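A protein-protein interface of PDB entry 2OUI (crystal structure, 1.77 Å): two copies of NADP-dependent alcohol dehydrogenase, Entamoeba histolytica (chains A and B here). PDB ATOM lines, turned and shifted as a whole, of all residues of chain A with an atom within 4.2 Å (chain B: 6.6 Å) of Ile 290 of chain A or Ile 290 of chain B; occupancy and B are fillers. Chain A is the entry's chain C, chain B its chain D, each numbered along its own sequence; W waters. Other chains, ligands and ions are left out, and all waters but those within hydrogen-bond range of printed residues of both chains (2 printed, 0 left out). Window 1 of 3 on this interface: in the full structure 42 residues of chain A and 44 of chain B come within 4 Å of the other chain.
A ring nitrogen (ND1) of His 291 of chain B lies within hydrogen-bond range of a ring nitrogen (ND1) of His 289 of chain A (2.9 Å).
O of Ile 290 of chain A is in hydrogen-bond range of N of Ile 290 of chain B, at 2.9 Å.
A ring nitrogen (ND1) of His 289 of chain B sits at hydrogen-bond distance from a ring nitrogen (ND1) of His 291 of chain A.
The backbone NH (N) of Ile 262 of chain A lies within hydrogen-bond range of the backbone carbonyl oxygen (O) of His 289 of chain A (2.9 Å).
The indole nitrogen (NE1) of Trp 281 of chain A lies within hydrogen-bond range of the backbone carbonyl oxygen (O) of Lys 288 of chain A (2.8 Å).
OD1 of Asp 261 of chain B sits at hydrogen-bond distance from NE2 of His 291 of chain B, 2.7 Å away.
The backbone carbonyl oxygen (O) of Ile 262 of chain B is in hydrogen-bond range of the backbone NH (N) of His 291 of chain B (2.8 Å).
The backbone carbonyl oxygen (O) of His 291 of chain B is in hydrogen-bond range of the backbone NH (N) of Asn 264 of chain B, 2.8 Å away.
The indole nitrogen (NE1) of Trp 281 of chain B lies within hydrogen-bond range of the backbone carbonyl oxygen (O) of Lys 288 of chain B, 2.8 Å away.
Ile 276 of chain A touches Ile 276 of chain B (CG1 to CG1, 3.99 Å).
CZ3 of Trp 281 of chain A touches CE2 of Phe 249 of chain B, at 3.7 Å.
Ile 290 of chain B touches Trp 281 of chain A.
C of His 291 of chain B touches CH2 of Trp 281 of chain A (3.9 Å).
Trp 281 of chain A touches Gly 292 of chain B (CH2 to CA, 3.7 Å).
His 289 of chain A touches Ile 290 of chain B.
CH2 of Trp 281 of chain B touches CG2 of Ile 290 of chain A, at 3.9 Å.
His 289 of chain B touches Ile 290 of chain A (CA to O, 3.6 Å).
Trp 281 of chain B touches His 291 of chain A.
Ile 290 of chain B touches just these residues of chain A: Trp 281 (3.8 Å), His 289 (3.7 Å) and Ile 290 (2.9 Å).
Of the printed residues of chain A, His 291 of chain B touches Trp 281 (3.9 Å) and His 289 (2.9 Å).
Of the printed residues of chain A, Phe 249 of chain B touches Trp 281 (3.7 Å).
Of the printed residues of chain A, Gly 292 of chain B touches Trp 281 (3.7 Å).
The nearest printed residue of chain A that does not touch His 289 of chain B is His 289 of chain A (6.7 Å).
Printed residues of chain A that touch a printed residue of chain B: Ile 276, Trp 281, His 289, Ile 290 and His 291.
Hydrophobic or aromatic side chains of chain B that line the printed part of chain A: Phe 249, Ile 276, Trp 281, His 289, Ile 290 and His 291.
Along chain B the printed residues that touch a printed residue of chain A span positions 249 to 292.
Among the printed residues, no Asp or Glu carboxylate lies within 4 Å of a Lys or Arg side-chain nitrogen of the other chain.
Ile 276 of chain B touches its own counterpart, Ile 276 of chain A.
Trp 281 of chain A touches His 291 of chain B, and with the chains exchanged His 291 of chain A touches Trp 281 of chain B.
His 289 of chain A touches Ile 290 of chain B, and with the chains exchanged Ile 290 of chain A touches His 289 of chain B.
His 289 of chain A touches His 291 of chain B, and with the chains exchanged His 291 of chain A touches His 289 of chain B.
Positions printed for both chains: 262, 276, 281, 288, 289, 290 and 291.
Of the 12 pairs that touch across the chains among the printed residues, 10 have their exchanged pair printed and touching as well.
Water W1 lies within hydrogen-bond range of the backbone NH of Gly 292 of chain B, a ring nitrogen (ND1) of His 289 of chain A and the backbone carbonyl oxygen of Lys 288 of chain A.
Water W2 lies within hydrogen-bond range of the backbone carbonyl oxygen (O) of Gly 292 of chain B (3.0 Å), the backbone NH (N) of Lys 288 of chain A (3.0 Å) and the indole nitrogen (NE1) of Trp 281 of chain A (3.1 Å).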
ATOM      1  N   ILE A 262      15.927   6.502 -21.141  1.00  0.00           N
ATOM      2  CA  ILE A 262      14.475   6.398 -21.109  1.00  0.00           C
ATOM      3  C   ILE A 262      13.955   7.823 -21.290  1.00  0.00           C
ATOM      4  O   ILE A 262      14.280   8.715 -20.492  1.00  0.00           O
ATOM      5  CB  ILE A 262      14.024   5.871 -19.746  1.00  0.00           C
ATOM      6  CG1 ILE A 262      14.492   4.428 -19.552  1.00  0.00           C
ATOM      7  CG2 ILE A 262      12.488   5.943 -19.632  1.00  0.00           C
ATOM      8  CD1 ILE A 262      14.370   3.932 -18.114  1.00  0.00           C
ATOM      9  N   ILE A 276      11.402   4.041  -8.968  1.00  0.00           N
ATOM     10  CA  ILE A 276      12.457   3.470  -9.821  1.00  0.00           C
ATOM     11  C   ILE A 276      13.029   2.257  -9.088  1.00  0.00           C
ATOM     12  O   ILE A 276      13.499   2.391  -7.946  1.00  0.00           O
ATOM     13  CB  ILE A 276      13.560   4.508 -10.089  1.00  0.00           C
ATOM     14  CG1 ILE A 276      12.960   5.789 -10.699  1.00  0.00           C
ATOM     15  CG2 ILE A 276      14.675   3.903 -10.964  1.00  0.00           C
ATOM     16  CD1 ILE A 276      12.070   5.550 -11.962  1.00  0.00           C
ATOM     17  N   TRP A 281      17.851  -0.850 -11.594  1.00  0.00           N
ATOM     18  CA  TRP A 281      18.523   0.390 -11.958  1.00  0.00           C
ATOM     19  C   TRP A 281      20.026   0.282 -11.650  1.00  0.00           C
ATOM     20  O   TRP A 281      20.733   1.288 -11.569  1.00  0.00           O
ATOM     21  CB  TRP A 281      17.868   1.588 -11.237  1.00  0.00           C
ATOM     22  CG  TRP A 281      18.089   2.908 -11.966  1.00  0.00           C
ATOM     23  CD1 TRP A 281      17.814   3.183 -13.270  1.00  0.00           C
ATOM     24  CD2 TRP A 281      18.637   4.110 -11.402  1.00  0.00           C
ATOM     25  NE1 TRP A 281      18.152   4.512 -13.561  1.00  0.00           N
ATOM     26  CE2 TRP A 281      18.645   5.091 -12.416  1.00  0.00           C
ATOM     27  CE3 TRP A 281      19.110   4.450 -10.115  1.00  0.00           C
ATOM     28  CZ2 TRP A 281      19.161   6.380 -12.208  1.00  0.00           C
ATOM     29  CZ3 TRP A 281      19.594   5.741  -9.896  1.00  0.00           C
ATOM     30  CH2 TRP A 281      19.612   6.689 -10.942  1.00  0.00           C
ATOM     31  N   LYS A 288      21.318   3.893 -16.654  1.00  0.00           N
ATOM     32  CA  LYS A 288      19.994   3.900 -17.290  1.00  0.00           C
ATOM     33  C   LYS A 288      19.438   5.289 -17.064  1.00  0.00           C
ATOM     34  O   LYS A 288      18.835   5.572 -16.014  1.00  0.00           O
ATOM     35  CB  LYS A 288      19.090   2.813 -16.664  1.00  0.00           C
ATOM     36  CG  LYS A 288      19.534   1.385 -17.073  1.00  0.00           C
ATOM     37  CD  LYS A 288      18.720   0.296 -16.363  1.00  0.00           C
ATOM     38  CE  LYS A 288      19.088  -1.091 -16.910  1.00  0.00           C
ATOM     39  NZ  LYS A 288      18.147  -2.115 -16.390  1.00  0.00           N
ATOM     40  N   HIS A 289      19.751   6.187 -17.988  1.00  0.00           N
ATOM     41  CA  HIS A 289      19.467   7.628 -17.787  1.00  0.00           C
ATOM     42  C   HIS A 289      17.971   7.885 -17.904  1.00  0.00           C
ATOM     43  O   HIS A 289      17.319   7.362 -18.797  1.00  0.00           O
ATOM     44  CB  HIS A 289      20.203   8.488 -18.819  1.00  0.00           C
ATOM     45  CG  HIS A 289      21.682   8.242 -18.859  1.00  0.00           C
ATOM     46  ND1 HIS A 289      22.528   8.618 -17.837  1.00  0.00           N
ATOM     47  CD2 HIS A 289      22.467   7.681 -19.812  1.00  0.00           C
ATOM     48  CE1 HIS A 289      23.772   8.295 -18.154  1.00  0.00           C
ATOM     49  NE2 HIS A 289      23.762   7.722 -19.347  1.00  0.00           N
ATOM     50  N   ILE A 290      17.418   8.663 -16.976  1.00  0.00           N
ATOM     51  CA  ILE A 290      15.973   8.875 -16.965  1.00  0.00           C
ATOM     52  C   ILE A 290      15.694  10.354 -17.288  1.00  0.00           C
ATOM     53  O   ILE A 290      16.163  11.249 -16.565  1.00  0.00           O
ATOM     54  CB  ILE A 290      15.372   8.513 -15.608  1.00  0.00           C
ATOM     55  CG1 ILE A 290      15.592   7.014 -15.291  1.00  0.00           C
ATOM     56  CG2 ILE A 290      13.864   8.807 -15.594  1.00  0.00           C
ATOM     57  CD1 ILE A 290      15.371   6.676 -13.822  1.00  0.00           C
ATOM     58  N   HIS A 291      14.931  10.570 -18.356  1.00  0.00           N
ATOM     59  CA  HIS A 291      14.600  11.917 -18.868  1.00  0.00           C
ATOM     60  C   HIS A 291      13.081  12.050 -18.860  1.00  0.00           C
ATOM     61  O   HIS A 291      12.342  11.069 -19.084  1.00  0.00           O
ATOM     62  CB  HIS A 291      15.128  12.100 -20.297  1.00  0.00           C
ATOM     63  CG  HIS A 291      16.559  11.666 -20.485  1.00  0.00           C
ATOM     64  ND1 HIS A 291      17.637  12.420 -20.059  1.00  0.00           N
ATOM     65  CD2 HIS A 291      17.083  10.552 -21.046  1.00  0.00           C
ATOM     66  CE1 HIS A 291      18.761  11.795 -20.363  1.00  0.00           C
ATOM     67  NE2 HIS A 291      18.455  10.651 -20.952  1.00  0.00           N
ATOM     68  N   PHE B 249      17.305  11.054  -3.551  1.00  0.00           N
ATOM     69  CA  PHE B 249      16.927  11.498  -4.878  1.00  0.00           C
ATOM     70  C   PHE B 249      15.794  12.514  -4.843  1.00  0.00           C
ATOM     71  O   PHE B 249      15.820  13.476  -5.598  1.00  0.00           O
ATOM     72  CB  PHE B 249      16.563  10.305  -5.750  1.00  0.00           C
ATOM     73  CG  PHE B 249      17.739   9.484  -6.121  1.00  0.00           C
ATOM     74  CD1 PHE B 249      18.342   8.626  -5.175  1.00  0.00           C
ATOM     75  CD2 PHE B 249      18.277   9.564  -7.401  1.00  0.00           C
ATOM     76  CE1 PHE B 249      19.458   7.869  -5.515  1.00  0.00           C
ATOM     77  CE2 PHE B 249      19.388   8.799  -7.747  1.00  0.00           C
ATOM     78  CZ  PHE B 249      19.976   7.941  -6.788  1.00  0.00           C
ATOM     79  N   VAL B 253      15.797  16.295  -6.396  1.00  0.00           N
ATOM     80  CA  VAL B 253      14.756  16.777  -7.308  1.00  0.00           C
ATOM     81  C   VAL B 253      14.148  18.052  -6.772  1.00  0.00           C
ATOM     82  O   VAL B 253      13.918  19.003  -7.523  1.00  0.00           O
ATOM     83  CB  VAL B 253      13.668  15.704  -7.573  1.00  0.00           C
ATOM     84  CG1 VAL B 253      12.430  16.291  -8.298  1.00  0.00           C
ATOM     85  CG2 VAL B 253      14.274  14.561  -8.342  1.00  0.00           C
ATOM     86  N   SER B 260      18.046  20.474 -15.948  1.00  0.00           N
ATOM     87  CA  SER B 260      19.170  20.237 -15.055  1.00  0.00           C
ATOM     88  C   SER B 260      19.553  18.767 -15.016  1.00  0.00           C
ATOM     89  O   SER B 260      18.926  17.957 -15.684  1.00  0.00           O
ATOM     90  CB  SER B 260      18.797  20.702 -13.649  1.00  0.00           C
ATOM     91  OG  SER B 260      17.718  19.927 -13.169  1.00  0.00           O
ATOM     92  N   ASP B 261      20.613  18.459 -14.260  1.00  0.00           N
ATOM     93  CA  ASP B 261      21.132  17.108 -14.149  1.00  0.00           C
ATOM     94  C   ASP B 261      21.446  16.736 -12.701  1.00  0.00           C
ATOM     95  O   ASP B 261      22.017  17.530 -11.950  1.00  0.00           O
ATOM     96  CB  ASP B 261      22.370  16.948 -15.026  1.00  0.00           C
ATOM     97  CG  ASP B 261      22.069  17.165 -16.489  1.00  0.00           C
ATOM     98  OD1 ASP B 261      21.796  16.155 -17.161  1.00  0.00           O
ATOM     99  OD2 ASP B 261      22.108  18.335 -16.964  1.00  0.00           O
ATOM    100  N   ILE B 262      21.034  15.527 -12.329  1.00  0.00           N
ATOM    101  CA  ILE B 262      21.378  14.923 -11.049  1.00  0.00           C
ATOM    102  C   ILE B 262      22.292  13.750 -11.341  1.00  0.00           C
ATOM    103  O   ILE B 262      21.892  12.822 -12.062  1.00  0.00           O
ATOM    104  CB  ILE B 262      20.106  14.433 -10.323  1.00  0.00           C
ATOM    105  CG1 ILE B 262      19.181  15.620 -10.014  1.00  0.00           C
ATOM    106  CG2 ILE B 262      20.461  13.606  -9.080  1.00  0.00           C
ATOM    107  CD1 ILE B 262      17.724  15.198  -9.741  1.00  0.00           C
ATOM    108  N   GLY B 263      23.511  13.802 -10.802  1.00  0.00           N
ATOM    109  CA  GLY B 263      24.487  12.750 -11.036  1.00  0.00           C
ATOM    110  C   GLY B 263      24.689  11.904  -9.796  1.00  0.00           C
ATOM    111  O   GLY B 263      25.384  12.318  -8.871  1.00  0.00           O
ATOM    112  N   ASN B 264      24.101  10.717  -9.774  1.00  0.00           N
ATOM    113  CA  ASN B 264      24.344   9.822  -8.651  1.00  0.00           C
ATOM    114  C   ASN B 264      25.506   8.864  -8.895  1.00  0.00           C
ATOM    115  O   ASN B 264      25.610   8.236  -9.955  1.00  0.00           O
ATOM    116  CB  ASN B 264      23.116   8.997  -8.339  1.00  0.00           C
ATOM    117  CG  ASN B 264      23.402   7.964  -7.256  1.00  0.00           C
ATOM    118  OD1 ASN B 264      23.657   8.344  -6.109  1.00  0.00           O
ATOM    119  ND2 ASN B 264      23.441   6.674  -7.628  1.00  0.00           N
ATOM    120  N   ILE B 276      10.777   9.071  -6.912  1.00  0.00           N
ATOM    121  CA  ILE B 276      10.941  10.402  -7.539  1.00  0.00           C
ATOM    122  C   ILE B 276       9.623  11.171  -7.392  1.00  0.00           C
ATOM    123  O   ILE B 276       8.585  10.707  -7.882  1.00  0.00           O
ATOM    124  CB  ILE B 276      11.348  10.256  -9.015  1.00  0.00           C
ATOM    125  CG1 ILE B 276      12.651   9.445  -9.126  1.00  0.00           C
ATOM    126  CG2 ILE B 276      11.457  11.642  -9.708  1.00  0.00           C
ATOM    127  CD1 ILE B 276      13.852  10.043  -8.330  1.00  0.00           C
ATOM    128  N   TRP B 281       9.064  16.803  -9.908  1.00  0.00           N
ATOM    129  CA  TRP B 281       9.728  16.369 -11.134  1.00  0.00           C
ATOM    130  C   TRP B 281       9.016  16.968 -12.364  1.00  0.00           C
ATOM    131  O   TRP B 281       9.224  16.513 -13.491  1.00  0.00           O
ATOM    132  CB  TRP B 281       9.810  14.844 -11.225  1.00  0.00           C
ATOM    133  CG  TRP B 281      10.954  14.328 -12.107  1.00  0.00           C
ATOM    134  CD1 TRP B 281      12.277  14.625 -11.988  1.00  0.00           C
ATOM    135  CD2 TRP B 281      10.855  13.410 -13.220  1.00  0.00           C
ATOM    136  NE1 TRP B 281      13.013  13.960 -12.952  1.00  0.00           N
ATOM    137  CE2 TRP B 281      12.162  13.210 -13.717  1.00  0.00           C
ATOM    138  CE3 TRP B 281       9.784  12.744 -13.842  1.00  0.00           C
ATOM    139  CZ2 TRP B 281      12.432  12.377 -14.815  1.00  0.00           C
ATOM    140  CZ3 TRP B 281      10.051  11.909 -14.928  1.00  0.00           C
ATOM    141  CH2 TRP B 281      11.362  11.734 -15.400  1.00  0.00           C
ATOM    142  N   LYS B 288      14.462  17.425 -15.448  1.00  0.00           N
ATOM    143  CA  LYS B 288      15.401  17.186 -14.370  1.00  0.00           C
ATOM    144  C   LYS B 288      15.978  15.798 -14.616  1.00  0.00           C
ATOM    145  O   LYS B 288      15.443  14.787 -14.148  1.00  0.00           O
ATOM    146  CB  LYS B 288      14.660  17.251 -13.029  1.00  0.00           C
ATOM    147  CG  LYS B 288      14.338  18.686 -12.636  1.00  0.00           C
ATOM    148  CD  LYS B 288      13.468  18.792 -11.385  1.00  0.00           C
ATOM    149  CE  LYS B 288      13.309  20.256 -11.053  1.00  0.00           C
ATOM    150  NZ  LYS B 288      12.688  20.429  -9.710  1.00  0.00           N
ATOM    151  N   HIS B 289      17.028  15.750 -15.425  1.00  0.00           N
ATOM    152  CA  HIS B 289      17.586  14.500 -15.871  1.00  0.00           C
ATOM    153  C   HIS B 289      18.205  13.739 -14.707  1.00  0.00           C
ATOM    154  O   HIS B 289      18.994  14.288 -13.929  1.00  0.00           O
ATOM    155  CB  HIS B 289      18.648  14.771 -16.916  1.00  0.00           C
ATOM    156  CG  HIS B 289      18.159  15.624 -18.049  1.00  0.00           C
ATOM    157  ND1 HIS B 289      17.181  15.188 -18.910  1.00  0.00           N
ATOM    158  CD2 HIS B 289      18.511  16.866 -18.470  1.00  0.00           C
ATOM    159  CE1 HIS B 289      16.960  16.120 -19.826  1.00  0.00           C
ATOM    160  NE2 HIS B 289      17.753  17.146 -19.583  1.00  0.00           N
ATOM    161  N   ILE B 290      17.879  12.462 -14.608  1.00  0.00           N
ATOM    162  CA  ILE B 290      18.422  11.659 -13.504  1.00  0.00           C
ATOM    163  C   ILE B 290      19.434  10.643 -14.022  1.00  0.00           C
ATOM    164  O   ILE B 290      19.115   9.835 -14.887  1.00  0.00           O
ATOM    165  CB  ILE B 290      17.308  10.928 -12.760  1.00  0.00           C
ATOM    166  CG1 ILE B 290      16.325  11.934 -12.140  1.00  0.00           C
ATOM    167  CG2 ILE B 290      17.879  10.042 -11.638  1.00  0.00           C
ATOM    168  CD1 ILE B 290      15.027  11.301 -11.740  1.00  0.00           C
ATOM    169  N   HIS B 291      20.660  10.720 -13.524  1.00  0.00           N
ATOM    170  CA  HIS B 291      21.704   9.791 -13.949  1.00  0.00           C
ATOM    171  C   HIS B 291      22.232   9.014 -12.731  1.00  0.00           C
ATOM    172  O   HIS B 291      22.276   9.542 -11.588  1.00  0.00           O
ATOM    173  CB  HIS B 291      22.858  10.526 -14.638  1.00  0.00           C
ATOM    174  CG  HIS B 291      22.438  11.602 -15.592  1.00  0.00           C
ATOM    175  ND1 HIS B 291      22.163  11.363 -16.925  1.00  0.00           N
ATOM    176  CD2 HIS B 291      22.311  12.943 -15.417  1.00  0.00           C
ATOM    177  CE1 HIS B 291      21.844  12.503 -17.515  1.00  0.00           C
ATOM    178  NE2 HIS B 291      21.926  13.474 -16.624  1.00  0.00           N
ATOM    179  N   GLY B 292      22.581   7.750 -12.943  1.00  0.00           N
ATOM    180  CA  GLY B 292      23.182   6.962 -11.877  1.00  0.00           C
ATOM    181  C   GLY B 292      24.187   6.030 -12.525  1.00  0.00           C
ATOM    182  O   GLY B 292      23.787   5.116 -13.255  1.00  0.00           O
HETATM  183  O   HOH W   1      21.777   6.925 -15.431  1.00  0.00           O
HETATM  184  O   HOH W   2      21.196   3.722 -13.653  1.00  0.00           O
